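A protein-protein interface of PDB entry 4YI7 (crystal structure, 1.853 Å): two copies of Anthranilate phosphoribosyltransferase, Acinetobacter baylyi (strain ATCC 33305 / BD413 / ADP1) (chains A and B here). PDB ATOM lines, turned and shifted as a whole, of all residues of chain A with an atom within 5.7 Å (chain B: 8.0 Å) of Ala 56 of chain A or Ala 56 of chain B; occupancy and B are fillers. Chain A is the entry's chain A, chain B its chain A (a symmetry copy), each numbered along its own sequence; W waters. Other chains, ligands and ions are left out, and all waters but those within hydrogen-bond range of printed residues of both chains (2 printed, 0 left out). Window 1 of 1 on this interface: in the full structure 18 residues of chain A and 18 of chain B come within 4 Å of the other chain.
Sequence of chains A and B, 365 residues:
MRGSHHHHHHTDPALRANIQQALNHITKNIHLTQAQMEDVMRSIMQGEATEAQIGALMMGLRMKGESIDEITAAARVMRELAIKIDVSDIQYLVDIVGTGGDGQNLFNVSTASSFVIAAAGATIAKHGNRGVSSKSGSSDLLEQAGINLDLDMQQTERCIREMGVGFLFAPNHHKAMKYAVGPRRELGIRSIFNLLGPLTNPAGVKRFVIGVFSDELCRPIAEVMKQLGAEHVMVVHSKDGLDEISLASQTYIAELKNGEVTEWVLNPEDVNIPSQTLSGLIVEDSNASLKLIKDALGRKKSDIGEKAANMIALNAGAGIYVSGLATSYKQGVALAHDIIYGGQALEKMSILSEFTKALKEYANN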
ATOM      1  N   LEU A  23     -23.884   2.896 -24.841  1.00  0.00           N
ATOM      2  CA  LEU A  23     -23.011   2.848 -26.004  1.00  0.00           C
ATOM      3  C   LEU A  23     -23.265   1.588 -26.828  1.00  0.00           C
ATOM      4  O   LEU A  23     -23.231   1.639 -28.049  1.00  0.00           O
ATOM      5  CB  LEU A  23     -21.537   2.929 -25.579  1.00  0.00           C
ATOM      6  CG  LEU A  23     -21.053   4.309 -25.132  1.00  0.00           C
ATOM      7  CD1 LEU A  23     -19.649   4.223 -24.539  1.00  0.00           C
ATOM      8  CD2 LEU A  23     -21.076   5.284 -26.292  1.00  0.00           C
ATOM      9  N   GLU A  51     -13.749  11.020 -20.590  1.00  0.00           N
ATOM     10  CA  GLU A  51     -13.625  11.778 -21.820  1.00  0.00           C
ATOM     11  C   GLU A  51     -13.805  10.879 -23.039  1.00  0.00           C
ATOM     12  O   GLU A  51     -14.481  11.261 -23.994  1.00  0.00           O
ATOM     13  CB  GLU A  51     -12.277  12.487 -21.870  1.00  0.00           C
ATOM     14  CG  GLU A  51     -12.033  13.385 -20.658  1.00  0.00           C
ATOM     15  CD  GLU A  51     -11.251  14.630 -21.002  1.00  0.00           C
ATOM     16  OE1 GLU A  51     -10.185  14.510 -21.643  1.00  0.00           O
ATOM     17  OE2 GLU A  51     -11.710  15.732 -20.632  1.00  0.00           O
ATOM     18  N   ALA A  52     -13.214   9.685 -22.997  1.00  0.00           N
ATOM     19  CA  ALA A  52     -13.397   8.708 -24.069  1.00  0.00           C
ATOM     20  C   ALA A  52     -14.879   8.369 -24.224  1.00  0.00           C
ATOM     21  O   ALA A  52     -15.388   8.267 -25.336  1.00  0.00           O
ATOM     22  CB  ALA A  52     -12.579   7.440 -23.787  1.00  0.00           C
ATOM     23  N   GLN A  53     -15.573   8.208 -23.103  1.00  0.00           N
ATOM     24  CA  GLN A  53     -16.988   7.857 -23.126  1.00  0.00           C
ATOM     25  C   GLN A  53     -17.844   8.987 -23.685  1.00  0.00           C
ATOM     26  O   GLN A  53     -18.839   8.753 -24.364  1.00  0.00           O
ATOM     27  CB  GLN A  53     -17.476   7.513 -21.730  1.00  0.00           C
ATOM     28  CG  GLN A  53     -17.078   6.131 -21.241  1.00  0.00           C
ATOM     29  CD  GLN A  53     -17.460   5.914 -19.792  1.00  0.00           C
ATOM     30  OE1 GLN A  53     -17.805   6.864 -19.069  1.00  0.00           O
ATOM     31  NE2 GLN A  53     -17.420   4.662 -19.359  1.00  0.00           N
ATOM     32  N   ILE A  54     -17.464  10.218 -23.371  1.00  0.00           N
ATOM     33  CA  ILE A  54     -18.176  11.374 -23.894  1.00  0.00           C
ATOM     34  C   ILE A  54     -17.970  11.496 -25.393  1.00  0.00           C
ATOM     35  O   ILE A  54     -18.914  11.750 -26.134  1.00  0.00           O
ATOM     36  CB  ILE A  54     -17.720  12.656 -23.196  1.00  0.00           C
ATOM     37  CG1 ILE A  54     -18.127  12.589 -21.722  1.00  0.00           C
ATOM     38  CG2 ILE A  54     -18.318  13.879 -23.896  1.00  0.00           C
ATOM     39  CD1 ILE A  54     -17.470  13.661 -20.837  1.00  0.00           C
ATOM     40  N   GLY A  55     -16.733  11.295 -25.837  1.00  0.00           N
ATOM     41  CA  GLY A  55     -16.426  11.331 -27.254  1.00  0.00           C
ATOM     42  C   GLY A  55     -17.224  10.278 -28.000  1.00  0.00           C
ATOM     43  O   GLY A  55     -17.779  10.552 -29.069  1.00  0.00           O
ATOM     44  N   ALA A  56     -17.280   9.071 -27.430  1.00  0.00           N
ATOM     45  CA  ALA A  56     -18.029   7.958 -28.027  1.00  0.00           C
ATOM     46  C   ALA A  56     -19.535   8.236 -28.097  1.00  0.00           C
ATOM     47  O   ALA A  56     -20.188   7.954 -29.107  1.00  0.00           O
ATOM     48  CB  ALA A  56     -17.771   6.666 -27.237  1.00  0.00           C
ATOM     49  N   LEU A  57     -20.089   8.791 -27.023  1.00  0.00           N
ATOM     50  CA  LEU A  57     -21.507   9.109 -26.995  1.00  0.00           C
ATOM     51  C   LEU A  57     -21.856  10.147 -28.054  1.00  0.00           C
ATOM     52  O   LEU A  57     -22.821   9.971 -28.782  1.00  0.00           O
ATOM     53  CB  LEU A  57     -21.918   9.621 -25.618  1.00  0.00           C
ATOM     54  CG  LEU A  57     -22.042   8.542 -24.544  1.00  0.00           C
ATOM     55  CD1 LEU A  57     -21.969   9.155 -23.161  1.00  0.00           C
ATOM     56  CD2 LEU A  57     -23.331   7.748 -24.734  1.00  0.00           C
ATOM     57  N   MET A  58     -21.065  11.216 -28.139  1.00  0.00           N
ATOM     58  CA  MET A  58     -21.275  12.258 -29.152  1.00  0.00           C
ATOM     59  C   MET A  58     -21.235  11.702 -30.584  1.00  0.00           C
ATOM     60  O   MET A  58     -22.123  11.970 -31.404  1.00  0.00           O
ATOM     61  CB  MET A  58     -20.223  13.351 -29.031  1.00  0.00           C
ATOM     62  CG  MET A  58     -20.294  14.178 -27.780  1.00  0.00           C
ATOM     63  SD  MET A  58     -18.829  15.185 -27.515  1.00  0.00           S
ATOM     64  CE  MET A  58     -18.741  16.155 -29.010  1.00  0.00           C
ATOM     65  N   MET A  59     -20.179  10.950 -30.884  1.00  0.00           N
ATOM     66  CA  MET A  59     -20.016  10.371 -32.207  1.00  0.00           C
ATOM     67  C   MET A  59     -21.142   9.401 -32.534  1.00  0.00           C
ATOM     68  O   MET A  59     -21.750   9.467 -33.609  1.00  0.00           O
ATOM     69  CB  MET A  59     -18.677   9.638 -32.305  1.00  0.00           C
ATOM     70  CG  MET A  59     -18.256   9.375 -33.716  1.00  0.00           C
ATOM     71  SD  MET A  59     -17.726  10.877 -34.533  1.00  0.00           S
ATOM     72  CE  MET A  59     -16.974  10.130 -35.982  1.00  0.00           C
ATOM     73  N   GLY A  60     -21.410   8.490 -31.603  1.00  0.00           N
ATOM     74  CA  GLY A  60     -22.404   7.450 -31.811  1.00  0.00           C
ATOM     75  C   GLY A  60     -23.819   7.985 -31.995  1.00  0.00           C
ATOM     76  O   GLY A  60     -24.547   7.564 -32.907  1.00  0.00           O
ATOM     77  N   LEU A  61     -24.214   8.911 -31.125  1.00  0.00           N
ATOM     78  CA  LEU A  61     -25.528   9.551 -31.239  1.00  0.00           C
ATOM     79  C   LEU A  61     -25.662  10.311 -32.547  1.00  0.00           C
ATOM     80  O   LEU A  61     -26.725  10.310 -33.151  1.00  0.00           O
ATOM     81  CB  LEU A  61     -25.771  10.494 -30.060  1.00  0.00           C
ATOM     82  CG  LEU A  61     -25.965   9.815 -28.707  1.00  0.00           C
ATOM     83  CD1 LEU A  61     -25.897  10.834 -27.580  1.00  0.00           C
ATOM     84  CD2 LEU A  61     -27.296   9.059 -28.679  1.00  0.00           C
ATOM     85  N   LEU A 187     -13.057  16.817 -30.743  1.00  0.00           N
ATOM     86  CA  LEU A 187     -13.718  16.085 -31.820  1.00  0.00           C
ATOM     87  C   LEU A 187     -13.952  16.986 -33.020  1.00  0.00           C
ATOM     88  O   LEU A 187     -13.740  16.589 -34.163  1.00  0.00           O
ATOM     89  CB  LEU A 187     -15.051  15.493 -31.344  1.00  0.00           C
ATOM     90  CG  LEU A 187     -15.026  14.063 -30.801  1.00  0.00           C
ATOM     91  CD1 LEU A 187     -14.064  13.922 -29.624  1.00  0.00           C
ATOM     92  CD2 LEU A 187     -16.447  13.619 -30.418  1.00  0.00           C
ATOM     93  N   ILE B  19      -7.006  14.278 -37.348  1.00  0.00           N
ATOM     94  CA  ILE B  19      -7.971  13.480 -36.596  1.00  0.00           C
ATOM     95  C   ILE B  19      -9.380  14.082 -36.695  1.00  0.00           C
ATOM     96  O   ILE B  19     -10.360  13.364 -36.873  1.00  0.00           O
ATOM     97  CB  ILE B  19      -7.533  13.362 -35.121  1.00  0.00           C
ATOM     98  CG1 ILE B  19      -6.309  12.439 -35.036  1.00  0.00           C
ATOM     99  CG2 ILE B  19      -8.667  12.834 -34.244  1.00  0.00           C
ATOM    100  CD1 ILE B  19      -5.657  12.401 -33.673  1.00  0.00           C
ATOM    101  N   LEU B  23     -12.577  12.312 -38.333  1.00  0.00           N
ATOM    102  CA  LEU B  23     -13.846  12.169 -37.634  1.00  0.00           C
ATOM    103  C   LEU B  23     -14.992  12.753 -38.456  1.00  0.00           C
ATOM    104  O   LEU B  23     -16.079  12.193 -38.473  1.00  0.00           O
ATOM    105  CB  LEU B  23     -13.780  12.833 -36.250  1.00  0.00           C
ATOM    106  CG  LEU B  23     -12.982  12.071 -35.191  1.00  0.00           C
ATOM    107  CD1 LEU B  23     -12.811  12.919 -33.932  1.00  0.00           C
ATOM    108  CD2 LEU B  23     -13.659  10.758 -34.854  1.00  0.00           C
ATOM    109  N   ILE B  26     -15.883  10.337 -41.277  1.00  0.00           N
ATOM    110  CA  ILE B  26     -16.561   9.185 -40.702  1.00  0.00           C
ATOM    111  C   ILE B  26     -18.033   9.481 -40.411  1.00  0.00           C
ATOM    112  O   ILE B  26     -18.870   8.603 -40.615  1.00  0.00           O
ATOM    113  CB  ILE B  26     -15.857   8.706 -39.407  1.00  0.00           C
ATOM    114  CG1 ILE B  26     -14.496   8.091 -39.747  1.00  0.00           C
ATOM    115  CG2 ILE B  26     -16.696   7.657 -38.685  1.00  0.00           C
ATOM    116  CD1 ILE B  26     -13.577   7.909 -38.549  1.00  0.00           C
ATOM    117  N   THR B  27     -18.364  10.690 -39.948  1.00  0.00           N
ATOM    118  CA  THR B  27     -19.779  11.021 -39.696  1.00  0.00           C
ATOM    119  C   THR B  27     -20.563  11.074 -41.009  1.00  0.00           C
ATOM    120  O   THR B  27     -21.778  10.887 -41.019  1.00  0.00           O
ATOM    121  CB  THR B  27     -19.993  12.383 -38.965  1.00  0.00           C
ATOM    122  OG1 THR B  27     -19.519  13.467 -39.777  1.00  0.00           O
ATOM    123  CG2 THR B  27     -19.310  12.407 -37.596  1.00  0.00           C
ATOM    124  N   THR B  50      -6.267  12.537 -28.277  1.00  0.00           N
ATOM    125  CA  THR B  50      -6.898  12.652 -26.977  1.00  0.00           C
ATOM    126  C   THR B  50      -7.823  11.473 -26.721  1.00  0.00           C
ATOM    127  O   THR B  50      -8.264  10.812 -27.657  1.00  0.00           O
ATOM    128  CB  THR B  50      -7.721  13.962 -26.861  1.00  0.00           C
ATOM    129  OG1 THR B  50      -8.918  13.834 -27.636  1.00  0.00           O
ATOM    130  CG2 THR B  50      -6.901  15.167 -27.353  1.00  0.00           C
ATOM    131  N   GLU B  51      -8.135  11.230 -25.453  1.00  0.00           N
ATOM    132  CA  GLU B  51      -8.989  10.119 -25.082  1.00  0.00           C
ATOM    133  C   GLU B  51     -10.376  10.262 -25.703  1.00  0.00           C
ATOM    134  O   GLU B  51     -10.934   9.283 -26.199  1.00  0.00           O
ATOM    135  CB  GLU B  51      -9.089  10.013 -23.565  1.00  0.00           C
ATOM    136  CG  GLU B  51      -7.725   9.892 -22.888  1.00  0.00           C
ATOM    137  CD  GLU B  51      -7.758   9.009 -21.663  1.00  0.00           C
ATOM    138  OE1 GLU B  51      -8.630   9.223 -20.793  1.00  0.00           O
ATOM    139  OE2 GLU B  51      -6.911   8.095 -21.576  1.00  0.00           O
ATOM    140  N   ALA B  52     -10.918  11.479 -25.688  1.00  0.00           N
ATOM    141  CA  ALA B  52     -12.200  11.749 -26.338  1.00  0.00           C
ATOM    142  C   ALA B  52     -12.116  11.412 -27.825  1.00  0.00           C
ATOM    143  O   ALA B  52     -13.034  10.824 -28.390  1.00  0.00           O
ATOM    144  CB  ALA B  52     -12.608  13.215 -26.137  1.00  0.00           C
ATOM    145  N   GLN B  53     -11.005  11.775 -28.456  1.00  0.00           N
ATOM    146  CA  GLN B  53     -10.823  11.530 -29.882  1.00  0.00           C
ATOM    147  C   GLN B  53     -10.706  10.043 -30.193  1.00  0.00           C
ATOM    148  O   GLN B  53     -11.170   9.573 -31.227  1.00  0.00           O
ATOM    149  CB  GLN B  53      -9.580  12.239 -30.391  1.00  0.00           C
ATOM    150  CG  GLN B  53      -9.745  13.734 -30.606  1.00  0.00           C
ATOM    151  CD  GLN B  53      -8.433  14.400 -30.962  1.00  0.00           C
ATOM    152  OE1 GLN B  53      -7.350  13.806 -30.819  1.00  0.00           O
ATOM    153  NE2 GLN B  53      -8.515  15.632 -31.445  1.00  0.00           N
ATOM    154  N   ILE B  54     -10.059   9.308 -29.299  1.00  0.00           N
ATOM    155  CA  ILE B  54      -9.935   7.869 -29.466  1.00  0.00           C
ATOM    156  C   ILE B  54     -11.285   7.194 -29.312  1.00  0.00           C
ATOM    157  O   ILE B  54     -11.636   6.314 -30.093  1.00  0.00           O
ATOM    158  CB  ILE B  54      -8.940   7.287 -28.460  1.00  0.00           C
ATOM    159  CG1 ILE B  54      -7.545   7.832 -28.771  1.00  0.00           C
ATOM    160  CG2 ILE B  54      -8.977   5.757 -28.506  1.00  0.00           C
ATOM    161  CD1 ILE B  54      -6.507   7.579 -27.665  1.00  0.00           C
ATOM    162  N   GLY B  55     -12.049   7.623 -28.313  1.00  0.00           N
ATOM    163  CA  GLY B  55     -13.382   7.091 -28.102  1.00  0.00           C
ATOM    164  C   GLY B  55     -14.254   7.338 -29.319  1.00  0.00           C
ATOM    165  O   GLY B  55     -14.983   6.443 -29.759  1.00  0.00           O
ATOM    166  N   ALA B  56     -14.175   8.556 -29.861  1.00  0.00           N
ATOM    167  CA  ALA B  56     -14.947   8.934 -31.051  1.00  0.00           C
ATOM    168  C   ALA B  56     -14.553   8.118 -32.288  1.00  0.00           C
ATOM    169  O   ALA B  56     -15.412   7.671 -33.055  1.00  0.00           O
ATOM    170  CB  ALA B  56     -14.775  10.434 -31.336  1.00  0.00           C
ATOM    171  N   LEU B  57     -13.252   7.925 -32.485  1.00  0.00           N
ATOM    172  CA  LEU B  57     -12.776   7.151 -33.619  1.00  0.00           C
ATOM    173  C   LEU B  57     -13.263   5.710 -33.542  1.00  0.00           C
ATOM    174  O   LEU B  57     -13.756   5.182 -34.528  1.00  0.00           O
ATOM    175  CB  LEU B  57     -11.252   7.177 -33.689  1.00  0.00           C
ATOM    176  CG  LEU B  57     -10.656   8.484 -34.208  1.00  0.00           C
ATOM    177  CD1 LEU B  57      -9.204   8.609 -33.798  1.00  0.00           C
ATOM    178  CD2 LEU B  57     -10.818   8.578 -35.723  1.00  0.00           C
ATOM    179  N   MET B  58     -13.130   5.087 -32.372  1.00  0.00           N
ATOM    180  CA  MET B  58     -13.606   3.714 -32.166  1.00  0.00           C
ATOM    181  C   MET B  58     -15.108   3.563 -32.452  1.00  0.00           C
ATOM    182  O   MET B  58     -15.538   2.659 -33.180  1.00  0.00           O
ATOM    183  CB  MET B  58     -13.341   3.257 -30.738  1.00  0.00           C
ATOM    184  CG  MET B  58     -11.894   3.095 -30.372  1.00  0.00           C
ATOM    185  SD  MET B  58     -11.628   2.924 -28.603  1.00  0.00           S
ATOM    186  CE  MET B  58     -12.634   1.511 -28.186  1.00  0.00           C
ATOM    187  N   MET B  59     -15.905   4.441 -31.846  1.00  0.00           N
ATOM    188  CA  MET B  59     -17.345   4.402 -32.025  1.00  0.00           C
ATOM    189  C   MET B  59     -17.734   4.641 -33.477  1.00  0.00           C
ATOM    190  O   MET B  59     -18.533   3.895 -34.056  1.00  0.00           O
ATOM    191  CB  MET B  59     -18.020   5.457 -31.146  1.00  0.00           C
ATOM    192  CG  MET B  59     -19.484   5.215 -30.961  1.00  0.00           C
ATOM    193  SD  MET B  59     -19.788   3.822 -29.879  1.00  0.00           S
ATOM    194  CE  MET B  59     -21.544   4.085 -29.609  1.00  0.00           C
ATOM    195  N   GLY B  60     -17.170   5.695 -34.061  1.00  0.00           N
ATOM    196  CA  GLY B  60     -17.508   6.091 -35.418  1.00  0.00           C
ATOM    197  C   GLY B  60     -17.143   5.049 -36.468  1.00  0.00           C
ATOM    198  O   GLY B  60     -17.947   4.730 -37.358  1.00  0.00           O
ATOM    199  N   LEU B  61     -15.927   4.520 -36.373  1.00  0.00           N
ATOM    200  CA  LEU B  61     -15.484   3.459 -37.282  1.00  0.00           C
ATOM    201  C   LEU B  61     -16.347   2.217 -37.147  1.00  0.00           C
ATOM    202  O   LEU B  61     -16.640   1.563 -38.137  1.00  0.00           O
ATOM    203  CB  LEU B  61     -14.018   3.106 -37.025  1.00  0.00           C
ATOM    204  CG  LEU B  61     -13.007   4.181 -37.418  1.00  0.00           C
ATOM    205  CD1 LEU B  61     -11.633   3.858 -36.850  1.00  0.00           C
ATOM    206  CD2 LEU B  61     -12.948   4.322 -38.940  1.00  0.00           C
ATOM    207  N   ARG B  62     -16.764   1.892 -35.927  1.00  0.00           N
ATOM    208  CA  ARG B  62     -17.584   0.709 -35.713  1.00  0.00           C
ATOM    209  C   ARG B  62     -18.952   0.886 -36.364  1.00  0.00           C
ATOM    210  O   ARG B  62     -19.486  -0.036 -36.973  1.00  0.00           O
ATOM    211  CB  ARG B  62     -17.741   0.416 -34.223  1.00  0.00           C
ATOM    212  CG  ARG B  62     -18.513  -0.867 -33.883  1.00  0.00           C
ATOM    213  CD  ARG B  62     -17.680  -2.150 -34.065  1.00  0.00           C
ATOM    214  NE  ARG B  62     -17.362  -2.454 -35.456  1.00  0.00           N
ATOM    215  CZ  ARG B  62     -18.182  -3.082 -36.298  1.00  0.00           C
ATOM    216  NH1 ARG B  62     -19.404  -3.455 -35.913  1.00  0.00           N
ATOM    217  NH2 ARG B  62     -17.792  -3.309 -37.537  1.00  0.00           N
ATOM    218  N   MET B  63     -19.521   2.077 -36.243  1.00  0.00           N
ATOM    219  CA  MET B  63     -20.864   2.294 -36.775  1.00  0.00           C
ATOM    220  C   MET B  63     -20.876   2.470 -38.288  1.00  0.00           C
ATOM    221  O   MET B  63     -21.808   2.015 -38.952  1.00  0.00           O
ATOM    222  CB  MET B  63     -21.506   3.473 -36.069  1.00  0.00           C
ATOM    223  CG  MET B  63     -21.818   3.069 -34.660  1.00  0.00           C
ATOM    224  SD  MET B  63     -22.581   4.293 -33.684  1.00  0.00           S
ATOM    225  CE  MET B  63     -24.229   4.394 -34.422  1.00  0.00           C
ATOM    226  N   PRO B 183      -9.470   3.829 -23.012  1.00  0.00           N
ATOM    227  CA  PRO B 183     -10.677   4.018 -23.834  1.00  0.00           C
ATOM    228  C   PRO B 183     -11.407   2.695 -24.123  1.00  0.00           C
ATOM    229  O   PRO B 183     -12.632   2.639 -24.057  1.00  0.00           O
ATOM    230  CB  PRO B 183     -10.125   4.667 -25.105  1.00  0.00           C
ATOM    231  CG  PRO B 183      -8.922   5.429 -24.638  1.00  0.00           C
ATOM    232  CD  PRO B 183      -8.326   4.604 -23.519  1.00  0.00           C
ATOM    233  N   GLU B 186     -13.303   1.570 -20.952  1.00  0.00           N
ATOM    234  CA  GLU B 186     -14.351   2.549 -20.643  1.00  0.00           C
ATOM    235  C   GLU B 186     -15.547   2.457 -21.588  1.00  0.00           C
ATOM    236  O   GLU B 186     -16.696   2.518 -21.151  1.00  0.00           O
ATOM    237  CB  GLU B 186     -13.763   3.965 -20.685  1.00  0.00           C
ATOM    238  CG  GLU B 186     -12.754   4.235 -19.572  1.00  0.00           C
ATOM    239  CD  GLU B 186     -11.865   5.443 -19.819  1.00  0.00           C
ATOM    240  OE1 GLU B 186     -12.156   6.276 -20.709  1.00  0.00           O
ATOM    241  OE2 GLU B 186     -10.859   5.569 -19.100  1.00  0.00           O
ATOM    242  N   LEU B 187     -15.283   2.315 -22.887  1.00  0.00           N
ATOM    243  CA  LEU B 187     -16.367   2.204 -23.860  1.00  0.00           C
ATOM    244  C   LEU B 187     -17.058   0.856 -23.747  1.00  0.00           C
ATOM    245  O   LEU B 187     -18.281   0.764 -23.794  1.00  0.00           O
ATOM    246  CB  LEU B 187     -15.844   2.404 -25.289  1.00  0.00           C
ATOM    247  CG  LEU B 187     -15.891   3.824 -25.857  1.00  0.00           C
ATOM    248  CD1 LEU B 187     -15.110   4.807 -24.987  1.00  0.00           C
ATOM    249  CD2 LEU B 187     -15.376   3.830 -27.305  1.00  0.00           C
ATOM    250  N   GLY B 188     -16.258  -0.198 -23.612  1.00  0.00           N
ATOM    251  CA  GLY B 188     -16.788  -1.530 -23.450  1.00  0.00           C
ATOM    252  C   GLY B 188     -17.269  -2.164 -24.741  1.00  0.00           C
ATOM    253  O   GLY B 188     -17.793  -3.273 -24.714  1.00  0.00           O
ATOM    254  N   ILE B 189     -17.092  -1.481 -25.872  1.00  0.00           N
ATOM    255  CA  ILE B 189     -17.595  -1.998 -27.142  1.00  0.00           C
ATOM    256  C   ILE B 189     -16.531  -2.835 -27.847  1.00  0.00           C
ATOM    257  O   ILE B 189     -15.350  -2.718 -27.550  1.00  0.00           O
ATOM    258  CB  ILE B 189     -18.054  -0.861 -28.106  1.00  0.00           C
ATOM    259  CG1 ILE B 189     -16.886   0.047 -28.505  1.00  0.00           C
ATOM    260  CG2 ILE B 189     -19.150  -0.039 -27.466  1.00  0.00           C
ATOM    261  CD1 ILE B 189     -17.151   0.854 -29.747  1.00  0.00           C
HETATM  262  O   HOH W   1     -11.206   8.626 -21.006  1.00  0.00           O
HETATM  263  O   HOH W   2      -9.992  13.956 -24.230  1.00  0.00           O
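O of Glu 186 of chain B is in hydrogen-bond range of NE2 of Gln 53 of chain A (2.9 Å).
N of Thr 50 of chain B lies within hydrogen-bond range of OE1 of Gln 53 of chain B, 3.0 Å away.
Among the printed residues, pairs that only touch across the chains: Ala 52 of chain A with Glu 51 of chain B (3.3 Å), Glu 51 of chain A with Ala 52 of chain B (3.3 Å), Ala 52 of chain A with Glu 186 of chain B (3.3 Å), Met 59 of chain A with Leu 23 of chain B (3.4 Å), Leu 23 of chain A with Met 59 of chain B (3.4 Å), Met 59 of chain A with Ala 56 of chain B (3.4 Å), Ala 56 of chain A with Met 59 of chain B (3.4 Å), Ala 52 of chain A with Leu 187 of chain B (3.5 Å), Leu 187 of chain A with Ala 52 of chain B (3.5 Å), Gly 60 of chain A with Met 63 of chain B (3.5 Å), Gly 55 of chain A with Ala 52 of chain B (3.6 Å), Ala 52 of chain A with Gly 55 of chain B (3.6 Å), Met 59 of chain A with Thr 27 of chain B (3.6 Å), Met 59 of chain A with Ile 26 of chain B (3.7 Å), Ala 56 of chain A with Leu 187 of chain B (3.7 Å), Leu 187 of chain A with Ala 56 of chain B (3.7 Å), Gly 55 of chain A with Ala 56 of chain B (3.8 Å), Ala 56 of chain A with Gly 55 of chain B (3.8 Å), Met 59 of chain A with Gly 60 of chain B (3.8 Å), Gly 60 of chain A with Met 59 of chain B (3.8 Å), Leu 187 of chain A with Leu 23 of chain B (3.8 Å), Leu 23 of chain A with Leu 187 of chain B (3.8 Å), Ala 52 of chain A with Pro 183 of chain B (3.9 Å), Gln 53 of chain A with Leu 187 of chain B (3.9 Å), Leu 187 of chain A with Gln 53 of chain B (3.9 Å), Ala 52 of chain A with Ala 52 of chain B (3.97 Å) and Ala 56 of chain A with Ala 56 of chain B (3.98 Å).
Of chain A, only Gly 55, Ala 56, Met 59 and Leu 187 come within 4 Å of Ala 56 of chain B. Of the printed residues of chain B, Gly 55 of chain A touches Ala 52 (3.6 Å) and Ala 56 (3.8 Å). Of the printed residues of chain A, Pro 183 of chain B touches Ala 52. Of the printed residues of chain B, Leu 187 of chain A touches Leu 23, Ala 52, Gln 53 and Ala 56. Of the printed residues of chain A, Ala 52 of chain B touches Glu 51 (3.3 Å), Ala 52 (3.97 Å), Gly 55 (3.6 Å) and Leu 187 (3.5 Å). Of the printed residues of chain A, Leu 187 of chain B touches Leu 23 (3.8 Å), Ala 52 (3.5 Å), Gln 53 (3.9 Å) and Ala 56 (3.7 Å).
Hydrophobic or aromatic side chains of chain A within 4 Å of the printed part of chain B: Leu 23, Ala 52, Ala 56, Met 59 and Leu 187. Printed residues of chain B that touch a printed residue of chain A: Leu 23, Ile 26, Thr 27, Glu 51, Ala 52, Gln 53, Gly 55, Ala 56, Met 59, Gly 60, Met 63, Pro 183, Glu 186 and Leu 187. Among the printed residues, no Asp or Glu carboxylate lies within 4 Å of a Lys or Arg side-chain nitrogen of the other chain.
Leu 23 of chain A touches Met 59 of chain B, and with the chains exchanged Met 59 of chain A touches Leu 23 of chain B. Ala 52 of chain A touches Gly 55 of chain B, and with the chains exchanged Gly 55 of chain A touches Ala 52 of chain B. Ala 52 of chain A touches Leu 187 of chain B, and with the chains exchanged Leu 187 of chain A touches Ala 52 of chain B. Gly 55 of chain A touches Ala 56 of chain B, and with the chains exchanged Ala 56 of chain A touches Gly 55 of chain B. Of the 28 pairs that touch across the chains among the printed residues, 22 have their exchanged pair printed and touching as well.
Water W1 lies within hydrogen-bond range of OE1 of Glu 186 of chain B (2.6 Å), OE1 of Glu 51 of chain B (2.7 Å) and N of Ala 52 of chain A (3.0 Å). Water W2 lies within hydrogen-bond range of OE1 of Glu 51 of chain A and N of Ala 52 of chain B.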
